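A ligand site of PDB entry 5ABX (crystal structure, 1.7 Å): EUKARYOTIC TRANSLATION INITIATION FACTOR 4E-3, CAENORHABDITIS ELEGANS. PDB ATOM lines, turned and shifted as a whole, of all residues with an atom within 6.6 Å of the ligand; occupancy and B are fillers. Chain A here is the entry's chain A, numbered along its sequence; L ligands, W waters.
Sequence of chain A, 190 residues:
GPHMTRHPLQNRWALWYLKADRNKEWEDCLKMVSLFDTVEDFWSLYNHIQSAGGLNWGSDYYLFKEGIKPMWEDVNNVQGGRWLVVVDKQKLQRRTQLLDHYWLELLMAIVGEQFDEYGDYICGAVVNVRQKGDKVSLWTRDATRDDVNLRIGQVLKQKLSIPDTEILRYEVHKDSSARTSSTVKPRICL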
ATOM      1  N   LEU A  18      -2.837 -20.364  -3.878  1.00  0.00           N
ATOM      2  CA  LEU A  18      -1.652 -19.528  -3.837  1.00  0.00           C
ATOM      3  C   LEU A  18      -0.447 -20.435  -3.681  1.00  0.00           C
ATOM      4  O   LEU A  18      -0.366 -21.187  -2.715  1.00  0.00           O
ATOM      5  CB  LEU A  18      -1.724 -18.524  -2.692  1.00  0.00           C
ATOM      6  CG  LEU A  18      -0.601 -17.477  -2.699  1.00  0.00           C
ATOM      7  CD1 LEU A  18      -1.096 -16.191  -2.081  1.00  0.00           C
ATOM      8  CD2 LEU A  18       0.637 -17.973  -1.966  1.00  0.00           C
ATOM      9  N   GLU A  25       5.067 -10.548  -6.051  1.00  0.00           N
ATOM     10  CA  GLU A  25       4.253  -9.937  -5.005  1.00  0.00           C
ATOM     11  C   GLU A  25       3.146 -10.920  -4.634  1.00  0.00           C
ATOM     12  O   GLU A  25       2.757 -11.753  -5.466  1.00  0.00           O
ATOM     13  CB  GLU A  25       3.648  -8.603  -5.462  1.00  0.00           C
ATOM     14  CG  GLU A  25       4.612  -7.437  -5.450  1.00  0.00           C
ATOM     15  CD  GLU A  25       5.103  -7.073  -4.059  1.00  0.00           C
ATOM     16  OE1 GLU A  25       4.464  -7.486  -3.066  1.00  0.00           O
ATOM     17  OE2 GLU A  25       6.133  -6.377  -3.970  1.00  0.00           O
ATOM     18  N   TRP A  26       2.659 -10.808  -3.407  1.00  0.00           N
ATOM     19  CA  TRP A  26       1.629 -11.691  -2.876  1.00  0.00           C
ATOM     20  C   TRP A  26       0.446 -11.896  -3.814  1.00  0.00           C
ATOM     21  O   TRP A  26       0.085 -13.032  -4.115  1.00  0.00           O
ATOM     22  CB  TRP A  26       1.121 -11.152  -1.538  1.00  0.00           C
ATOM     23  CG  TRP A  26       0.066 -12.019  -0.958  1.00  0.00           C
ATOM     24  CD1 TRP A  26       0.249 -13.138  -0.192  1.00  0.00           C
ATOM     25  CD2 TRP A  26      -1.359 -11.877  -1.114  1.00  0.00           C
ATOM     26  NE1 TRP A  26      -0.958 -13.679   0.153  1.00  0.00           N
ATOM     27  CE2 TRP A  26      -1.956 -12.935  -0.408  1.00  0.00           C
ATOM     28  CE3 TRP A  26      -2.165 -10.957  -1.778  1.00  0.00           C
ATOM     29  CZ2 TRP A  26      -3.339 -13.091  -0.340  1.00  0.00           C
ATOM     30  CZ3 TRP A  26      -3.542 -11.118  -1.716  1.00  0.00           C
ATOM     31  CH2 TRP A  26      -4.115 -12.171  -1.006  1.00  0.00           C
ATOM     32  N   GLU A  27      -0.152 -10.806  -4.276  1.00  0.00           N
ATOM     33  CA  GLU A  27      -1.346 -10.906  -5.111  1.00  0.00           C
ATOM     34  C   GLU A  27      -1.072 -11.630  -6.429  1.00  0.00           C
ATOM     35  O   GLU A  27      -1.970 -12.207  -7.029  1.00  0.00           O
ATOM     36  CB  GLU A  27      -1.923  -9.511  -5.384  1.00  0.00           C
ATOM     37  CG  GLU A  27      -0.985  -8.537  -6.079  1.00  0.00           C
ATOM     38  CD  GLU A  27      -0.022  -7.828  -5.133  1.00  0.00           C
ATOM     39  OE1 GLU A  27       0.078  -8.204  -3.946  1.00  0.00           O
ATOM     40  OE2 GLU A  27       0.658  -6.871  -5.593  1.00  0.00           O
ATOM     41  N   GLY A  58       4.052 -22.735   2.562  1.00  0.00           N
ATOM     42  CA  GLY A  58       3.860 -21.425   1.979  1.00  0.00           C
ATOM     43  C   GLY A  58       2.696 -21.330   1.010  1.00  0.00           C
ATOM     44  O   GLY A  58       2.380 -20.241   0.530  1.00  0.00           O
ATOM     45  N   ASP A  60      -1.427 -21.805  -0.081  1.00  0.00           N
ATOM     46  CA  ASP A  60      -2.758 -21.552   0.490  1.00  0.00           C
ATOM     47  C   ASP A  60      -3.870 -22.096  -0.399  1.00  0.00           C
ATOM     48  O   ASP A  60      -3.741 -22.128  -1.634  1.00  0.00           O
ATOM     49  CB  ASP A  60      -3.059 -20.056   0.648  1.00  0.00           C
ATOM     50  CG  ASP A  60      -1.970 -19.262   1.333  1.00  0.00           C
ATOM     51  OD1 ASP A  60      -1.313 -19.761   2.273  1.00  0.00           O
ATOM     52  OD2 ASP A  60      -1.813 -18.072   0.954  1.00  0.00           O
ATOM     53  N   TYR A  62      -8.037 -20.885  -0.831  1.00  0.00           N
ATOM     54  CA  TYR A  62      -9.100 -19.949  -0.444  1.00  0.00           C
ATOM     55  C   TYR A  62     -10.400 -20.447  -1.065  1.00  0.00           C
ATOM     56  O   TYR A  62     -10.399 -20.823  -2.239  1.00  0.00           O
ATOM     57  CB  TYR A  62      -8.828 -18.519  -0.920  1.00  0.00           C
ATOM     58  CG  TYR A  62      -7.496 -17.932  -0.500  1.00  0.00           C
ATOM     59  CD1 TYR A  62      -6.314 -18.294  -1.133  1.00  0.00           C
ATOM     60  CD2 TYR A  62      -7.446 -16.989   0.510  1.00  0.00           C
ATOM     61  CE1 TYR A  62      -5.103 -17.738  -0.731  1.00  0.00           C
ATOM     62  CE2 TYR A  62      -6.242 -16.435   0.906  1.00  0.00           C
ATOM     63  CZ  TYR A  62      -5.085 -16.816   0.285  1.00  0.00           C
ATOM     64  OH  TYR A  62      -3.910 -16.246   0.705  1.00  0.00           O
ATOM     65  N   PRO A  70     -10.226 -12.938  -2.557  1.00  0.00           N
ATOM     66  CA  PRO A  70      -9.717 -13.241  -1.217  1.00  0.00           C
ATOM     67  C   PRO A  70      -8.575 -12.317  -0.815  1.00  0.00           C
ATOM     68  O   PRO A  70      -7.433 -12.740  -0.589  1.00  0.00           O
ATOM     69  CB  PRO A  70      -9.264 -14.699  -1.346  1.00  0.00           C
ATOM     70  CG  PRO A  70      -8.855 -14.839  -2.759  1.00  0.00           C
ATOM     71  CD  PRO A  70      -9.774 -13.932  -3.550  1.00  0.00           C
ATOM     72  N   MET A  71      -8.909 -11.036  -0.727  1.00  0.00           N
ATOM     73  CA  MET A  71      -7.960  -9.977  -0.430  1.00  0.00           C
ATOM     74  C   MET A  71      -8.580  -8.987   0.557  1.00  0.00           C
ATOM     75  O   MET A  71      -9.757  -8.666   0.425  1.00  0.00           O
ATOM     76  CB  MET A  71      -7.566  -9.220  -1.697  1.00  0.00           C
ATOM     77  CG  MET A  71      -7.198 -10.085  -2.870  1.00  0.00           C
ATOM     78  SD  MET A  71      -7.060  -9.052  -4.347  1.00  0.00           S
ATOM     79  CE  MET A  71      -6.075 -10.127  -5.389  1.00  0.00           C
ATOM     80  N   TRP A  72      -7.779  -8.506   1.505  1.00  0.00           N
ATOM     81  CA  TRP A  72      -8.204  -7.448   2.418  1.00  0.00           C
ATOM     82  C   TRP A  72      -8.788  -6.265   1.647  1.00  0.00           C
ATOM     83  O   TRP A  72      -9.728  -5.622   2.096  1.00  0.00           O
ATOM     84  CB  TRP A  72      -7.040  -6.943   3.279  1.00  0.00           C
ATOM     85  CG  TRP A  72      -6.317  -7.983   4.059  1.00  0.00           C
ATOM     86  CD1 TRP A  72      -6.846  -9.070   4.705  1.00  0.00           C
ATOM     87  CD2 TRP A  72      -4.903  -8.027   4.305  1.00  0.00           C
ATOM     88  NE1 TRP A  72      -5.856  -9.787   5.324  1.00  0.00           N
ATOM     89  CE2 TRP A  72      -4.654  -9.161   5.094  1.00  0.00           C
ATOM     90  CE3 TRP A  72      -3.840  -7.218   3.923  1.00  0.00           C
ATOM     91  CZ2 TRP A  72      -3.372  -9.508   5.508  1.00  0.00           C
ATOM     92  CZ3 TRP A  72      -2.571  -7.560   4.335  1.00  0.00           C
ATOM     93  CH2 TRP A  72      -2.346  -8.699   5.120  1.00  0.00           C
ATOM     94  N   GLU A  73      -8.201  -5.997   0.479  1.00  0.00           N
ATOM     95  CA  GLU A  73      -8.553  -4.832  -0.316  1.00  0.00           C
ATOM     96  C   GLU A  73      -9.889  -4.947  -1.054  1.00  0.00           C
ATOM     97  O   GLU A  73     -10.411  -3.936  -1.547  1.00  0.00           O
ATOM     98  CB  GLU A  73      -7.453  -4.550  -1.350  1.00  0.00           C
ATOM     99  CG  GLU A  73      -6.099  -4.184  -0.743  1.00  0.00           C
ATOM    100  CD  GLU A  73      -5.339  -5.380  -0.193  1.00  0.00           C
ATOM    101  OE1 GLU A  73      -5.734  -6.538  -0.472  1.00  0.00           O
ATOM    102  OE2 GLU A  73      -4.333  -5.157   0.521  1.00  0.00           O
ATOM    103  N   ARG A  82     -11.360 -11.964  10.328  1.00  0.00           N
ATOM    104  CA  ARG A  82     -11.326 -13.413  10.277  1.00  0.00           C
ATOM    105  C   ARG A  82     -11.316 -14.047  11.652  1.00  0.00           C
ATOM    106  O   ARG A  82     -10.713 -13.505  12.597  1.00  0.00           O
ATOM    107  CB  ARG A  82     -10.098 -13.887   9.495  1.00  0.00           C
ATOM    108  CG  ARG A  82      -8.771 -13.549  10.160  1.00  0.00           C
ATOM    109  CD  ARG A  82      -7.588 -14.206   9.496  1.00  0.00           C
ATOM    110  NE  ARG A  82      -6.339 -13.906  10.186  1.00  0.00           N
ATOM    111  CZ  ARG A  82      -5.150 -14.407   9.865  1.00  0.00           C
ATOM    112  NH1 ARG A  82      -5.043 -15.254   8.840  1.00  0.00           N
ATOM    113  NH2 ARG A  82      -4.070 -14.068  10.557  1.00  0.00           N
ATOM    114  N   ASN A 128      -3.726 -21.852   5.364  1.00  0.00           N
ATOM    115  CA  ASN A 128      -2.327 -21.547   5.101  1.00  0.00           C
ATOM    116  C   ASN A 128      -1.483 -22.696   5.604  1.00  0.00           C
ATOM    117  O   ASN A 128      -1.594 -23.078   6.769  1.00  0.00           O
ATOM    118  CB  ASN A 128      -1.869 -20.266   5.814  1.00  0.00           C
ATOM    119  CG  ASN A 128      -2.790 -19.100   5.592  1.00  0.00           C
ATOM    120  OD1 ASN A 128      -3.411 -18.607   6.543  1.00  0.00           O
ATOM    121  ND2 ASN A 128      -2.822 -18.587   4.372  1.00  0.00           N
ATOM    122  N   ARG A 130       2.078 -23.769   6.703  1.00  0.00           N
ATOM    123  CA  ARG A 130       3.288 -23.085   7.152  1.00  0.00           C
ATOM    124  C   ARG A 130       4.059 -23.952   8.148  1.00  0.00           C
ATOM    125  O   ARG A 130       3.460 -24.629   8.983  1.00  0.00           O
ATOM    126  CB  ARG A 130       2.950 -21.747   7.807  1.00  0.00           C
ATOM    127  CG  ARG A 130       2.132 -20.776   6.949  1.00  0.00           C
ATOM    128  CD  ARG A 130       2.947 -20.152   5.833  1.00  0.00           C
ATOM    129  NE  ARG A 130       2.190 -19.099   5.154  1.00  0.00           N
ATOM    130  CZ  ARG A 130       1.346 -19.300   4.141  1.00  0.00           C
ATOM    131  NH1 ARG A 130       1.145 -20.518   3.660  1.00  0.00           N
ATOM    132  NH2 ARG A 130       0.710 -18.267   3.600  1.00  0.00           N
ATOM    133  N   LYS A 132       5.852 -22.979  10.654  1.00  0.00           N
ATOM    134  CA  LYS A 132       5.630 -22.462  12.001  1.00  0.00           C
ATOM    135  C   LYS A 132       4.310 -22.964  12.615  1.00  0.00           C
ATOM    136  O   LYS A 132       4.132 -22.949  13.829  1.00  0.00           O
ATOM    137  CB  LYS A 132       5.634 -20.932  11.986  1.00  0.00           C
ATOM    138  CG  LYS A 132       5.552 -20.286  13.358  1.00  0.00           C
ATOM    139  CD  LYS A 132       5.578 -18.765  13.283  1.00  0.00           C
ATOM    140  CE  LYS A 132       5.594 -18.151  14.677  1.00  0.00           C
ATOM    141  NZ  LYS A 132       5.333 -16.688  14.664  1.00  0.00           N
ATOM    142  N   GLY A 133       3.396 -23.404  11.755  1.00  0.00           N
ATOM    143  CA  GLY A 133       2.079 -23.825  12.197  1.00  0.00           C
ATOM    144  C   GLY A 133       1.046 -23.479  11.141  1.00  0.00           C
ATOM    145  O   GLY A 133       0.992 -22.352  10.668  1.00  0.00           O
ATOM    146  N   LYS A 135      -2.660 -22.710   9.496  1.00  0.00           N
ATOM    147  CA  LYS A 135      -3.756 -21.867   9.932  1.00  0.00           C
ATOM    148  C   LYS A 135      -4.994 -22.141   9.086  1.00  0.00           C
ATOM    149  O   LYS A 135      -4.887 -22.337   7.875  1.00  0.00           O
ATOM    150  CB  LYS A 135      -3.381 -20.385   9.864  1.00  0.00           C
ATOM    151  CG  LYS A 135      -2.280 -19.995  10.862  1.00  0.00           C
ATOM    152  CD  LYS A 135      -1.815 -18.558  10.702  1.00  0.00           C
ATOM    153  CE  LYS A 135      -0.966 -18.381   9.454  1.00  0.00           C
ATOM    154  NZ  LYS A 135      -0.436 -17.005   9.368  1.00  0.00           N
ATOM    155  N   TRP A 139     -13.239 -15.887   7.027  1.00  0.00           N
ATOM    156  CA  TRP A 139     -13.383 -14.456   6.781  1.00  0.00           C
ATOM    157  C   TRP A 139     -14.848 -14.029   6.779  1.00  0.00           C
ATOM    158  O   TRP A 139     -15.695 -14.660   6.127  1.00  0.00           O
ATOM    159  CB  TRP A 139     -12.735 -14.066   5.448  1.00  0.00           C
ATOM    160  CG  TRP A 139     -11.215 -14.100   5.396  1.00  0.00           C
ATOM    161  CD1 TRP A 139     -10.381 -14.914   6.113  1.00  0.00           C
ATOM    162  CD2 TRP A 139     -10.374 -13.287   4.570  1.00  0.00           C
ATOM    163  NE1 TRP A 139      -9.065 -14.640   5.781  1.00  0.00           N
ATOM    164  CE2 TRP A 139      -9.042 -13.644   4.840  1.00  0.00           C
ATOM    165  CE3 TRP A 139     -10.634 -12.276   3.632  1.00  0.00           C
ATOM    166  CZ2 TRP A 139      -7.962 -13.038   4.199  1.00  0.00           C
ATOM    167  CZ3 TRP A 139      -9.557 -11.678   2.996  1.00  0.00           C
ATOM    168  CH2 TRP A 139      -8.246 -12.060   3.290  1.00  0.00           C
ATOM    169  N   SER A 176      -4.546  -6.424  10.458  1.00  0.00           N
ATOM    170  CA  SER A 176      -3.652  -7.363   9.799  1.00  0.00           C
ATOM    171  C   SER A 176      -2.878  -6.690   8.672  1.00  0.00           C
ATOM    172  O   SER A 176      -1.743  -7.050   8.377  1.00  0.00           O
ATOM    173  CB  SER A 176      -4.451  -8.555   9.229  1.00  0.00           C
ATOM    174  OG  SER A 176      -5.140  -9.253  10.252  1.00  0.00           O
ATOM    175  N   SER A 177      -3.517  -5.707   8.046  1.00  0.00           N
ATOM    176  CA  SER A 177      -2.921  -4.976   6.925  1.00  0.00           C
ATOM    177  C   SER A 177      -1.823  -4.026   7.420  1.00  0.00           C
ATOM    178  O   SER A 177      -0.849  -3.780   6.708  1.00  0.00           O
ATOM    179  CB  SER A 177      -3.998  -4.203   6.169  1.00  0.00           C
ATOM    180  OG  SER A 177      -3.463  -3.571   5.027  1.00  0.00           O
HETATM  181  P1  LIG L   1      -0.331 -14.821   5.021  1.00  0.00           P
HETATM  182  O1  LIG L   1      -1.730 -14.138   5.260  1.00  0.00           O
HETATM  183  O2  LIG L   1      -0.422 -15.764   3.897  1.00  0.00           O
HETATM  184  O3  LIG L   1       0.141 -15.485   6.378  1.00  0.00           O
HETATM  185  O4  LIG L   1       0.771 -13.689   4.768  1.00  0.00           O
HETATM  186  P2  LIG L   1       1.609 -15.795   6.844  1.00  0.00           P
HETATM  187  O5  LIG L   1       1.560 -16.928   7.933  1.00  0.00           O
HETATM  188  O6  LIG L   1       2.452 -16.233   5.712  1.00  0.00           O
HETATM  189  O7  LIG L   1       2.105 -14.470   7.554  1.00  0.00           O
HETATM  190  P3  LIG L   1       3.168 -14.126   8.695  1.00  0.00           P
HETATM  191  O8  LIG L   1       4.551 -14.702   8.229  1.00  0.00           O
HETATM  192  O9  LIG L   1       3.183 -12.559   8.830  1.00  0.00           O
HETATM  193  O10 LIG L   1       2.821 -14.723  10.014  1.00  0.00           O
HETATM  194  C1  LIG L   1       0.695 -12.404   5.279  1.00  0.00           C
HETATM  195  C2  LIG L   1       1.506 -11.531   4.303  1.00  0.00           C
HETATM  196  O11 LIG L   1       1.072 -11.855   2.977  1.00  0.00           O
HETATM  197  C3  LIG L   1       1.271 -10.030   4.537  1.00  0.00           C
HETATM  198  O12 LIG L   1       2.428  -9.531   5.098  1.00  0.00           O
HETATM  199  C4  LIG L   1       1.133  -9.472   3.089  1.00  0.00           C
HETATM  200  O13 LIG L   1       2.404  -9.118   2.647  1.00  0.00           O
HETATM  201  C5  LIG L   1       0.628 -10.725   2.304  1.00  0.00           C
HETATM  202  N1  LIG L   1      -0.883 -10.797   2.312  1.00  0.00           N
HETATM  203  C6  LIG L   1      -1.699 -11.782   2.893  1.00  0.00           C
HETATM  204  N2  LIG L   1      -3.002 -11.478   2.662  1.00  0.00           N
HETATM  205  C7  LIG L   1      -4.166 -12.258   3.121  1.00  0.00           C
HETATM  206  C8  LIG L   1      -3.052 -10.297   1.910  1.00  0.00           C
HETATM  207  C9  LIG L   1      -4.169  -9.548   1.393  1.00  0.00           C
HETATM  208  O14 LIG L   1      -5.356  -9.809   1.473  1.00  0.00           O
HETATM  209  N3  LIG L   1      -3.765  -8.370   0.682  1.00  0.00           N
HETATM  210  C10 LIG L   1      -2.416  -8.026   0.529  1.00  0.00           C
HETATM  211  N4  LIG L   1      -2.117  -6.912  -0.181  1.00  0.00           N
HETATM  212  N5  LIG L   1      -1.351  -8.741   1.021  1.00  0.00           N
HETATM  213  C11 LIG L   1      -1.720  -9.854   1.701  1.00  0.00           C
HETATM  214  O   HOH W   1      -3.702 -15.991   3.503  1.00  0.00           O
HETATM  215  O   HOH W   2      -2.632 -16.208   7.766  1.00  0.00           O
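Merely in contact with the ligand: Met 71 (3.2 Å), Trp 26 (3.4 Å), Asn 128 (3.7 Å) and Asp 60 (3.99 Å). Hydrophobic or aromatic side chains that line the ligand: Trp 26, Met 71 and Trp 72. The nearest printed residue that does not touch the ligand is Trp 139 (4.02 Å).
N of Trp 72 sits at hydrogen-bond distance from O14 of the ligand. The side-chain amino group (NZ) of Lys 135 is in salt-bridge range of an oxygen (O5) of the ligand (2.5 Å). The guanidinium group of Arg 130 is in salt-bridge range of an oxygen (O2) of the ligand, 2.8 Å away. The side-chain carboxylate (OE2) of Glu 73 sits at hydrogen-bond distance from a nitrogen (N4) of the ligand, at 2.9 Å.
Water W2 lies within hydrogen-bond range of OD1 of Asn 128 (2.8 Å), NH1 of Arg 82 (2.8 Å), NZ of Lys 135 (2.8 Å) and O3 of the ligand (3.2 Å). Water W1 lies within hydrogen-bond range of OH of Tyr 62 (2.8 Å), ND2 of Asn 128 (2.9 Å) and O1 of the ligand (3.2 Å).
ND2 of Asn 128 sits at hydrogen-bond distance from OD1 of Asp 60, 2.8 Å away. The backbone carbonyl oxygen (O) of Leu 18 lies within hydrogen-bond range of the backbone NH (N) of Asp 60, 2.9 Å away. The guanidinium group (NH1) of Arg 130 sits close to the backbone carbonyl oxygen (O) of Gly 58. The backbone carbonyl oxygen (O) of Lys 135 is in hydrogen-bond range of the backbone NH (N) of Asn 128. The guanidinium group of Arg 130 lies within salt-bridge range of the side-chain carboxylate of Asp 60, at 2.8 Å. OH of Tyr 62 lies within hydrogen-bond range of OD2 of Asp 60 (2.8 Å).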
